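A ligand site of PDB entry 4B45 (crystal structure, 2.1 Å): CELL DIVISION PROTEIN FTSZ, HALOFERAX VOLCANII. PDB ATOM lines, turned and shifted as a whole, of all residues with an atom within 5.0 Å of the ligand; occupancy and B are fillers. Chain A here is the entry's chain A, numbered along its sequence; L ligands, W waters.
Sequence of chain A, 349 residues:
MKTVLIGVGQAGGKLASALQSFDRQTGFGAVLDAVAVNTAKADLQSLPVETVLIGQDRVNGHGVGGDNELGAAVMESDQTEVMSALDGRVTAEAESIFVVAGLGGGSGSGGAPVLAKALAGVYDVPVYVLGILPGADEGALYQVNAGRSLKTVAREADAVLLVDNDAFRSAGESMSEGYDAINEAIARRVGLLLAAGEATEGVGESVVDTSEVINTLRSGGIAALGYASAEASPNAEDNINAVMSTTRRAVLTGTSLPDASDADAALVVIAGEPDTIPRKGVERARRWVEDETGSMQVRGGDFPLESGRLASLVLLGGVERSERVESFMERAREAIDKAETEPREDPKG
Water W3 lies within hydrogen-bond range of O of Ile 132 (2.6 Å), N of Gly 104 (2.8 Å) and O11 of the ligand (3.1 Å). Water W1 bridges the side-chain hydroxyl of Tyr 142 (2.8 Å) and a sulfur (S1) of the ligand (3.4 Å).
The backbone NH (N) of Gln 10 lies close to the side-chain amide nitrogen (ND2) of Asn 38 (3.4 Å). The side-chain amide nitrogen (ND2) of Asn 183 lies close to the backbone carbonyl oxygen (O) of Tyr 179, at 3.3 Å.
Gly 9 touches the ligand. C of Val 64 touches O3 of the ligand (3.7 Å). CA of Gly 105 touches O8 of the ligand, 3.5 Å away. CD1 of Ile 132 touches N4 of the ligand (3.7 Å). CB of Pro 134 touches O11 of the ligand, 3.8 Å away. CG2 of Ile 182 touches N4 of the ligand, at 3.5 Å. Hydrophobic or aromatic side chains that line the ligand: Ala 11, Val 64, Ile 132, Pro 134, Tyr 179 and Ile 182. Within 4 Å of the ligand: Gly 9, Gln 10, Ala 11, Lys 14, Val 64, Gly 65, Gly 66, Gly 105, Gly 106, Ser 107, Gly 108, Ile 132, Pro 134, Glu 138, Asn 165, Tyr 179, Ile 182 and Asn 183. Along chain A the residues within 4 Å of the ligand span positions 9 to 183. The nearest printed residue that does not touch the ligand is Tyr 142 (4.1 Å).
NZ of Lys 14 is in hydrogen-bond range of O13 of the ligand. N of Gly 66 lies within hydrogen-bond range of O3 of the ligand (2.6 Å). The backbone NH (N) of Gln 10 is in hydrogen-bond range of an oxygen (O4) of the ligand (2.8 Å). OD1 of Asn 165 lies within hydrogen-bond range of N4 of the ligand (3.1 Å). O1 of the ligand sits at hydrogen-bond distance from N of Gly 106 (3.2 Å). O12 of the ligand is in hydrogen-bond range of OH of Tyr 179, at 2.8 Å. The side-chain amide oxygen (OD1) of Asn 183 sits at hydrogen-bond distance from a nitrogen (N3) of the ligand. OE1 of Glu 138 sits at hydrogen-bond distance from O11 of the ligand. N of Gly 65 sits at hydrogen-bond distance from O3 of the ligand (3.0 Å). The side-chain amide oxygen of Gln 10 sits close to a nitrogen (N2) of the ligand, at 3.1 Å. N of Ser 107 lies within hydrogen-bond range of O5 of the ligand, at 3.0 Å. N of Gly 108 sits at hydrogen-bond distance from O5 of the ligand. N of Ala 11 sits at hydrogen-bond distance from O7 of the ligand (2.7 Å).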
ATOM      1  N   VAL A   8       2.855 -23.671  10.389  1.00  0.00           N
ATOM      2  CA  VAL A   8       2.818 -25.105  10.080  1.00  0.00           C
ATOM      3  C   VAL A   8       4.215 -25.591   9.726  1.00  0.00           C
ATOM      4  O   VAL A   8       4.821 -25.139   8.761  1.00  0.00           O
ATOM      5  CB  VAL A   8       1.836 -25.422   8.944  1.00  0.00           C
ATOM      6  CG1 VAL A   8       1.838 -26.914   8.644  1.00  0.00           C
ATOM      7  CG2 VAL A   8       0.416 -24.975   9.308  1.00  0.00           C
ATOM      8  N   GLY A   9       4.741 -26.514  10.515  1.00  0.00           N
ATOM      9  CA  GLY A   9       6.119 -26.928  10.316  1.00  0.00           C
ATOM     10  C   GLY A   9       7.099 -26.037  11.054  1.00  0.00           C
ATOM     11  O   GLY A   9       6.739 -25.065  11.736  1.00  0.00           O
ATOM     12  N   GLN A  10       8.376 -26.366  10.909  1.00  0.00           N
ATOM     13  CA  GLN A  10       9.415 -25.731  11.709  1.00  0.00           C
ATOM     14  C   GLN A  10       9.659 -24.257  11.354  1.00  0.00           C
ATOM     15  O   GLN A  10       9.698 -23.382  12.232  1.00  0.00           O
ATOM     16  CB  GLN A  10      10.696 -26.543  11.589  1.00  0.00           C
ATOM     17  CG  GLN A  10      11.731 -26.148  12.596  1.00  0.00           C
ATOM     18  CD  GLN A  10      13.051 -25.901  11.940  1.00  0.00           C
ATOM     19  OE1 GLN A  10      13.178 -24.999  11.106  1.00  0.00           O
ATOM     20  NE2 GLN A  10      14.048 -26.701  12.291  1.00  0.00           N
ATOM     21  N   ALA A  11       9.870 -23.980  10.068  1.00  0.00           N
ATOM     22  CA  ALA A  11      10.066 -22.616   9.612  1.00  0.00           C
ATOM     23  C   ALA A  11       8.835 -21.762   9.933  1.00  0.00           C
ATOM     24  O   ALA A  11       8.948 -20.650  10.433  1.00  0.00           O
ATOM     25  CB  ALA A  11      10.337 -22.599   8.126  1.00  0.00           C
ATOM     26  N   GLY A  12       7.651 -22.307   9.646  1.00  0.00           N
ATOM     27  CA  GLY A  12       6.417 -21.590   9.896  1.00  0.00           C
ATOM     28  C   GLY A  12       6.232 -21.173  11.348  1.00  0.00           C
ATOM     29  O   GLY A  12       5.794 -20.058  11.640  1.00  0.00           O
ATOM     30  N   LYS A  14       8.621 -20.751  13.521  1.00  0.00           N
ATOM     31  CA  LYS A  14       9.653 -19.782  13.822  1.00  0.00           C
ATOM     32  C   LYS A  14       9.286 -18.374  13.311  1.00  0.00           C
ATOM     33  O   LYS A  14       9.439 -17.386  14.019  1.00  0.00           O
ATOM     34  CB  LYS A  14      11.003 -20.225  13.246  1.00  0.00           C
ATOM     35  CG  LYS A  14      11.768 -21.187  14.136  1.00  0.00           C
ATOM     36  CD  LYS A  14      13.274 -21.125  13.832  1.00  0.00           C
ATOM     37  CE  LYS A  14      13.794 -22.421  13.197  1.00  0.00           C
ATOM     38  NZ  LYS A  14      15.157 -22.287  12.569  1.00  0.00           N
ATOM     39  N   ASN A  38       2.889 -28.749  14.232  1.00  0.00           N
ATOM     40  CA  ASN A  38       4.039 -29.506  13.713  1.00  0.00           C
ATOM     41  C   ASN A  38       3.899 -30.975  14.027  1.00  0.00           C
ATOM     42  O   ASN A  38       2.992 -31.380  14.753  1.00  0.00           O
ATOM     43  CB  ASN A  38       5.334 -28.990  14.341  1.00  0.00           C
ATOM     44  CG  ASN A  38       6.524 -29.179  13.425  1.00  0.00           C
ATOM     45  OD1 ASN A  38       6.553 -30.076  12.580  1.00  0.00           O
ATOM     46  ND2 ASN A  38       7.518 -28.319  13.590  1.00  0.00           N
ATOM     47  N   ASP A  43      10.659 -29.218  17.877  1.00  0.00           N
ATOM     48  CA  ASP A  43      10.414 -27.911  17.280  1.00  0.00           C
ATOM     49  C   ASP A  43       9.417 -27.090  18.084  1.00  0.00           C
ATOM     50  O   ASP A  43       9.566 -25.875  18.219  1.00  0.00           O
ATOM     51  CB  ASP A  43       9.854 -28.067  15.858  1.00  0.00           C
ATOM     52  CG  ASP A  43      10.870 -28.628  14.902  1.00  0.00           C
ATOM     53  OD1 ASP A  43      12.047 -28.769  15.300  1.00  0.00           O
ATOM     54  OD2 ASP A  43      10.497 -28.920  13.739  1.00  0.00           O
ATOM     55  N   VAL A  64       8.269 -35.434   9.436  1.00  0.00           N
ATOM     56  CA  VAL A  64       8.008 -36.298   8.277  1.00  0.00           C
ATOM     57  C   VAL A  64       9.158 -36.320   7.281  1.00  0.00           C
ATOM     58  O   VAL A  64       9.031 -36.907   6.196  1.00  0.00           O
ATOM     59  CB  VAL A  64       6.697 -35.922   7.539  1.00  0.00           C
ATOM     60  CG1 VAL A  64       5.495 -35.941   8.509  1.00  0.00           C
ATOM     61  CG2 VAL A  64       6.816 -34.563   6.843  1.00  0.00           C
ATOM     62  N   GLY A  65      10.280 -35.695   7.645  1.00  0.00           N
ATOM     63  CA  GLY A  65      11.517 -35.827   6.893  1.00  0.00           C
ATOM     64  C   GLY A  65      11.425 -35.458   5.420  1.00  0.00           C
ATOM     65  O   GLY A  65      11.978 -36.141   4.560  1.00  0.00           O
ATOM     66  N   GLY A  66      10.688 -34.381   5.140  1.00  0.00           N
ATOM     67  CA  GLY A  66      10.658 -33.812   3.809  1.00  0.00           C
ATOM     68  C   GLY A  66       9.683 -34.529   2.909  1.00  0.00           C
ATOM     69  O   GLY A  66       9.632 -34.272   1.715  1.00  0.00           O
ATOM     70  N   ASP A  67       8.897 -35.435   3.492  1.00  0.00           N
ATOM     71  CA  ASP A  67       7.869 -36.163   2.754  1.00  0.00           C
ATOM     72  C   ASP A  67       6.592 -35.310   2.727  1.00  0.00           C
ATOM     73  O   ASP A  67       5.822 -35.287   3.692  1.00  0.00           O
ATOM     74  CB  ASP A  67       7.595 -37.509   3.435  1.00  0.00           C
ATOM     75  CG  ASP A  67       6.756 -38.456   2.577  1.00  0.00           C
ATOM     76  OD1 ASP A  67       5.888 -37.999   1.806  1.00  0.00           O
ATOM     77  OD2 ASP A  67       6.979 -39.681   2.692  1.00  0.00           O
ATOM     78  N   GLY A 102       7.108 -22.786   5.603  1.00  0.00           N
ATOM     79  CA  GLY A 102       8.204 -23.028   4.689  1.00  0.00           C
ATOM     80  C   GLY A 102       7.710 -23.967   3.611  1.00  0.00           C
ATOM     81  O   GLY A 102       7.290 -25.082   3.901  1.00  0.00           O
ATOM     82  N   GLY A 104       9.283 -25.540   1.241  1.00  0.00           N
ATOM     83  CA  GLY A 104      10.175 -26.617   0.831  1.00  0.00           C
ATOM     84  C   GLY A 104      10.198 -27.844   1.747  1.00  0.00           C
ATOM     85  O   GLY A 104      10.664 -28.908   1.343  1.00  0.00           O
ATOM     86  N   GLY A 105       9.718 -27.691   2.969  1.00  0.00           N
ATOM     87  CA  GLY A 105       9.752 -28.752   3.957  1.00  0.00           C
ATOM     88  C   GLY A 105       8.776 -29.880   3.651  1.00  0.00           C
ATOM     89  O   GLY A 105       8.320 -30.027   2.526  1.00  0.00           O
ATOM     90  N   GLY A 106       8.485 -30.698   4.645  1.00  0.00           N
ATOM     91  CA  GLY A 106       7.512 -31.766   4.471  1.00  0.00           C
ATOM     92  C   GLY A 106       6.202 -31.370   5.118  1.00  0.00           C
ATOM     93  O   GLY A 106       5.148 -31.450   4.489  1.00  0.00           O
ATOM     94  N   SER A 107       6.277 -30.904   6.359  1.00  0.00           N
ATOM     95  CA  SER A 107       5.085 -30.590   7.143  1.00  0.00           C
ATOM     96  C   SER A 107       4.360 -29.343   6.636  1.00  0.00           C
ATOM     97  O   SER A 107       3.158 -29.382   6.375  1.00  0.00           O
ATOM     98  CB  SER A 107       5.448 -30.402   8.620  1.00  0.00           C
ATOM     99  OG  SER A 107       5.673 -31.658   9.238  1.00  0.00           O
ATOM    100  N   GLY A 108       5.096 -28.242   6.504  1.00  0.00           N
ATOM    101  CA  GLY A 108       4.508 -27.007   6.028  1.00  0.00           C
ATOM    102  C   GLY A 108       4.043 -27.205   4.616  1.00  0.00           C
ATOM    103  O   GLY A 108       2.899 -26.921   4.280  1.00  0.00           O
ATOM    104  N   SER A 109       4.949 -27.713   3.783  1.00  0.00           N
ATOM    105  CA  SER A 109       4.659 -27.960   2.383  1.00  0.00           C
ATOM    106  C   SER A 109       3.372 -28.758   2.192  1.00  0.00           C
ATOM    107  O   SER A 109       2.482 -28.364   1.427  1.00  0.00           O
ATOM    108  CB  SER A 109       5.827 -28.708   1.757  1.00  0.00           C
ATOM    109  OG  SER A 109       5.524 -29.227   0.479  1.00  0.00           O
ATOM    110  N   ILE A 132       7.390 -19.333   2.669  1.00  0.00           N
ATOM    111  CA  ILE A 132       8.845 -19.187   2.493  1.00  0.00           C
ATOM    112  C   ILE A 132       9.391 -20.041   1.356  1.00  0.00           C
ATOM    113  O   ILE A 132       9.294 -21.283   1.369  1.00  0.00           O
ATOM    114  CB  ILE A 132       9.610 -19.536   3.781  1.00  0.00           C
ATOM    115  CG1 ILE A 132       9.265 -18.536   4.888  1.00  0.00           C
ATOM    116  CG2 ILE A 132      11.111 -19.542   3.536  1.00  0.00           C
ATOM    117  CD1 ILE A 132       9.347 -19.132   6.290  1.00  0.00           C
ATOM    118  N   PRO A 134      12.347 -21.703  -0.802  1.00  0.00           N
ATOM    119  CA  PRO A 134      13.694 -22.175  -0.446  1.00  0.00           C
ATOM    120  C   PRO A 134      14.739 -21.444  -1.259  1.00  0.00           C
ATOM    121  O   PRO A 134      14.486 -21.061  -2.397  1.00  0.00           O
ATOM    122  CB  PRO A 134      13.674 -23.653  -0.876  1.00  0.00           C
ATOM    123  CG  PRO A 134      12.662 -23.714  -1.962  1.00  0.00           C
ATOM    124  CD  PRO A 134      11.593 -22.701  -1.578  1.00  0.00           C
ATOM    125  N   GLU A 138      19.289 -24.914  -2.190  1.00  0.00           N
ATOM    126  CA  GLU A 138      18.679 -26.017  -1.446  1.00  0.00           C
ATOM    127  C   GLU A 138      18.422 -27.217  -2.345  1.00  0.00           C
ATOM    128  O   GLU A 138      18.306 -27.083  -3.566  1.00  0.00           O
ATOM    129  CB  GLU A 138      17.378 -25.570  -0.743  1.00  0.00           C
ATOM    130  CG  GLU A 138      17.613 -24.571   0.376  1.00  0.00           C
ATOM    131  CD  GLU A 138      16.354 -24.273   1.185  1.00  0.00           C
ATOM    132  OE1 GLU A 138      15.583 -25.216   1.470  1.00  0.00           O
ATOM    133  OE2 GLU A 138      16.130 -23.097   1.549  1.00  0.00           O
ATOM    134  N   TYR A 142      13.575 -30.216  -1.880  1.00  0.00           N
ATOM    135  CA  TYR A 142      12.971 -29.026  -1.316  1.00  0.00           C
ATOM    136  C   TYR A 142      12.402 -28.120  -2.417  1.00  0.00           C
ATOM    137  O   TYR A 142      11.360 -27.475  -2.229  1.00  0.00           O
ATOM    138  CB  TYR A 142      13.999 -28.279  -0.453  1.00  0.00           C
ATOM    139  CG  TYR A 142      14.594 -29.187   0.597  1.00  0.00           C
ATOM    140  CD1 TYR A 142      13.842 -29.585   1.694  1.00  0.00           C
ATOM    141  CD2 TYR A 142      15.889 -29.670   0.478  1.00  0.00           C
ATOM    142  CE1 TYR A 142      14.365 -30.421   2.662  1.00  0.00           C
ATOM    143  CE2 TYR A 142      16.436 -30.501   1.448  1.00  0.00           C
ATOM    144  CZ  TYR A 142      15.665 -30.878   2.533  1.00  0.00           C
ATOM    145  OH  TYR A 142      16.161 -31.707   3.506  1.00  0.00           O
ATOM    146  N   ASN A 165      14.074 -16.643   0.721  1.00  0.00           N
ATOM    147  CA  ASN A 165      15.203 -16.710   1.654  1.00  0.00           C
ATOM    148  C   ASN A 165      16.488 -16.161   1.045  1.00  0.00           C
ATOM    149  O   ASN A 165      17.301 -15.551   1.743  1.00  0.00           O
ATOM    150  CB  ASN A 165      15.446 -18.162   2.117  1.00  0.00           C
ATOM    151  CG  ASN A 165      14.565 -18.550   3.301  1.00  0.00           C
ATOM    152  OD1 ASN A 165      13.763 -17.731   3.777  1.00  0.00           O
ATOM    153  ND2 ASN A 165      14.706 -19.798   3.787  1.00  0.00           N
ATOM    154  N   TYR A 179      18.750 -17.422   9.424  1.00  0.00           N
ATOM    155  CA  TYR A 179      17.324 -17.694   9.527  1.00  0.00           C
ATOM    156  C   TYR A 179      16.634 -16.705  10.438  1.00  0.00           C
ATOM    157  O   TYR A 179      15.576 -16.202  10.110  1.00  0.00           O
ATOM    158  CB  TYR A 179      17.076 -19.109  10.048  1.00  0.00           C
ATOM    159  CG  TYR A 179      17.221 -20.188   9.005  1.00  0.00           C
ATOM    160  CD1 TYR A 179      16.747 -20.006   7.714  1.00  0.00           C
ATOM    161  CD2 TYR A 179      17.813 -21.407   9.331  1.00  0.00           C
ATOM    162  CE1 TYR A 179      16.873 -20.998   6.766  1.00  0.00           C
ATOM    163  CE2 TYR A 179      17.936 -22.413   8.388  1.00  0.00           C
ATOM    164  CZ  TYR A 179      17.465 -22.202   7.109  1.00  0.00           C
ATOM    165  OH  TYR A 179      17.599 -23.200   6.171  1.00  0.00           O
ATOM    166  N   ILE A 182      16.401 -13.379   8.669  1.00  0.00           N
ATOM    167  CA  ILE A 182      15.311 -13.379   7.682  1.00  0.00           C
ATOM    168  C   ILE A 182      13.974 -13.216   8.374  1.00  0.00           C
ATOM    169  O   ILE A 182      13.140 -12.408   7.975  1.00  0.00           O
ATOM    170  CB  ILE A 182      15.250 -14.674   6.881  1.00  0.00           C
ATOM    171  CG1 ILE A 182      16.535 -14.878   6.086  1.00  0.00           C
ATOM    172  CG2 ILE A 182      14.035 -14.665   5.959  1.00  0.00           C
ATOM    173  CD1 ILE A 182      16.657 -16.273   5.478  1.00  0.00           C
ATOM    174  N   ASN A 183      13.763 -13.996   9.420  1.00  0.00           N
ATOM    175  CA  ASN A 183      12.502 -13.960  10.134  1.00  0.00           C
ATOM    176  C   ASN A 183      12.237 -12.572  10.699  1.00  0.00           C
ATOM    177  O   ASN A 183      11.095 -12.077  10.682  1.00  0.00           O
ATOM    178  CB  ASN A 183      12.482 -14.988  11.257  1.00  0.00           C
ATOM    179  CG  ASN A 183      12.516 -16.403  10.757  1.00  0.00           C
ATOM    180  OD1 ASN A 183      12.257 -16.669   9.574  1.00  0.00           O
ATOM    181  ND2 ASN A 183      12.831 -17.323  11.638  1.00  0.00           N
HETATM  182  P1  LIG L   1      10.755 -31.436   7.455  1.00  0.00           P
HETATM  183  O1  LIG L   1       9.408 -30.617   7.756  1.00  0.00           O
HETATM  184  S1  LIG L   1      11.870 -30.782   5.837  1.00  0.00           S
HETATM  185  O2  LIG L   1      11.663 -31.432   8.722  1.00  0.00           O
HETATM  186  O3  LIG L   1      10.279 -32.778   7.094  1.00  0.00           O
HETATM  187  P2  LIG L   1       9.260 -29.034   7.955  1.00  0.00           P
HETATM  188  O4  LIG L   1       9.156 -28.612   9.393  1.00  0.00           O
HETATM  189  O5  LIG L   1       7.966 -28.616   7.252  1.00  0.00           O
HETATM  190  P3  LIG L   1      10.853 -26.770   7.546  1.00  0.00           P
HETATM  191  O6  LIG L   1      12.118 -26.603   8.348  1.00  0.00           O
HETATM  192  O7  LIG L   1       9.778 -25.940   8.205  1.00  0.00           O
HETATM  193  O8  LIG L   1      10.476 -28.267   7.322  1.00  0.00           O
HETATM  194  O9  LIG L   1      11.009 -26.160   6.126  1.00  0.00           O
HETATM  195  C1  LIG L   1      12.199 -26.183   5.415  1.00  0.00           C
HETATM  196  C2  LIG L   1      12.374 -24.976   4.592  1.00  0.00           C
HETATM  197  O10 LIG L   1      12.202 -23.822   5.365  1.00  0.00           O
HETATM  198  C3  LIG L   1      13.742 -24.878   4.030  1.00  0.00           C
HETATM  199  O11 LIG L   1      13.619 -24.177   2.854  1.00  0.00           O
HETATM  200  C4  LIG L   1      14.484 -24.078   4.999  1.00  0.00           C
HETATM  201  O12 LIG L   1      15.488 -23.375   4.349  1.00  0.00           O
HETATM  202  C5  LIG L   1      13.472 -23.147   5.473  1.00  0.00           C
HETATM  203  N1  LIG L   1      13.603 -22.720   6.854  1.00  0.00           N
HETATM  204  C6  LIG L   1      13.825 -23.503   7.921  1.00  0.00           C
HETATM  205  N2  LIG L   1      13.830 -22.738   9.033  1.00  0.00           N
HETATM  206  C7  LIG L   1      13.580 -21.448   8.662  1.00  0.00           C
HETATM  207  C8  LIG L   1      13.454 -20.231   9.400  1.00  0.00           C
HETATM  208  O13 LIG L   1      13.596 -20.201  10.775  1.00  0.00           O
HETATM  209  N3  LIG L   1      13.218 -19.092   8.717  1.00  0.00           N
HETATM  210  C9  LIG L   1      13.080 -19.101   7.377  1.00  0.00           C
HETATM  211  N4  LIG L   1      12.804 -17.828   6.702  1.00  0.00           N
HETATM  212  N5  LIG L   1      13.184 -20.224   6.634  1.00  0.00           N
HETATM  213  C10 LIG L   1      13.436 -21.420   7.279  1.00  0.00           C
HETATM  214  O   HOH W   1      14.049 -33.113   4.648  1.00  0.00           O
HETATM  215  O   HOH W   2       7.434 -24.588   7.853  1.00  0.00           O
HETATM  216  O   HOH W   3      10.852 -23.326   1.877  1.00  0.00           O
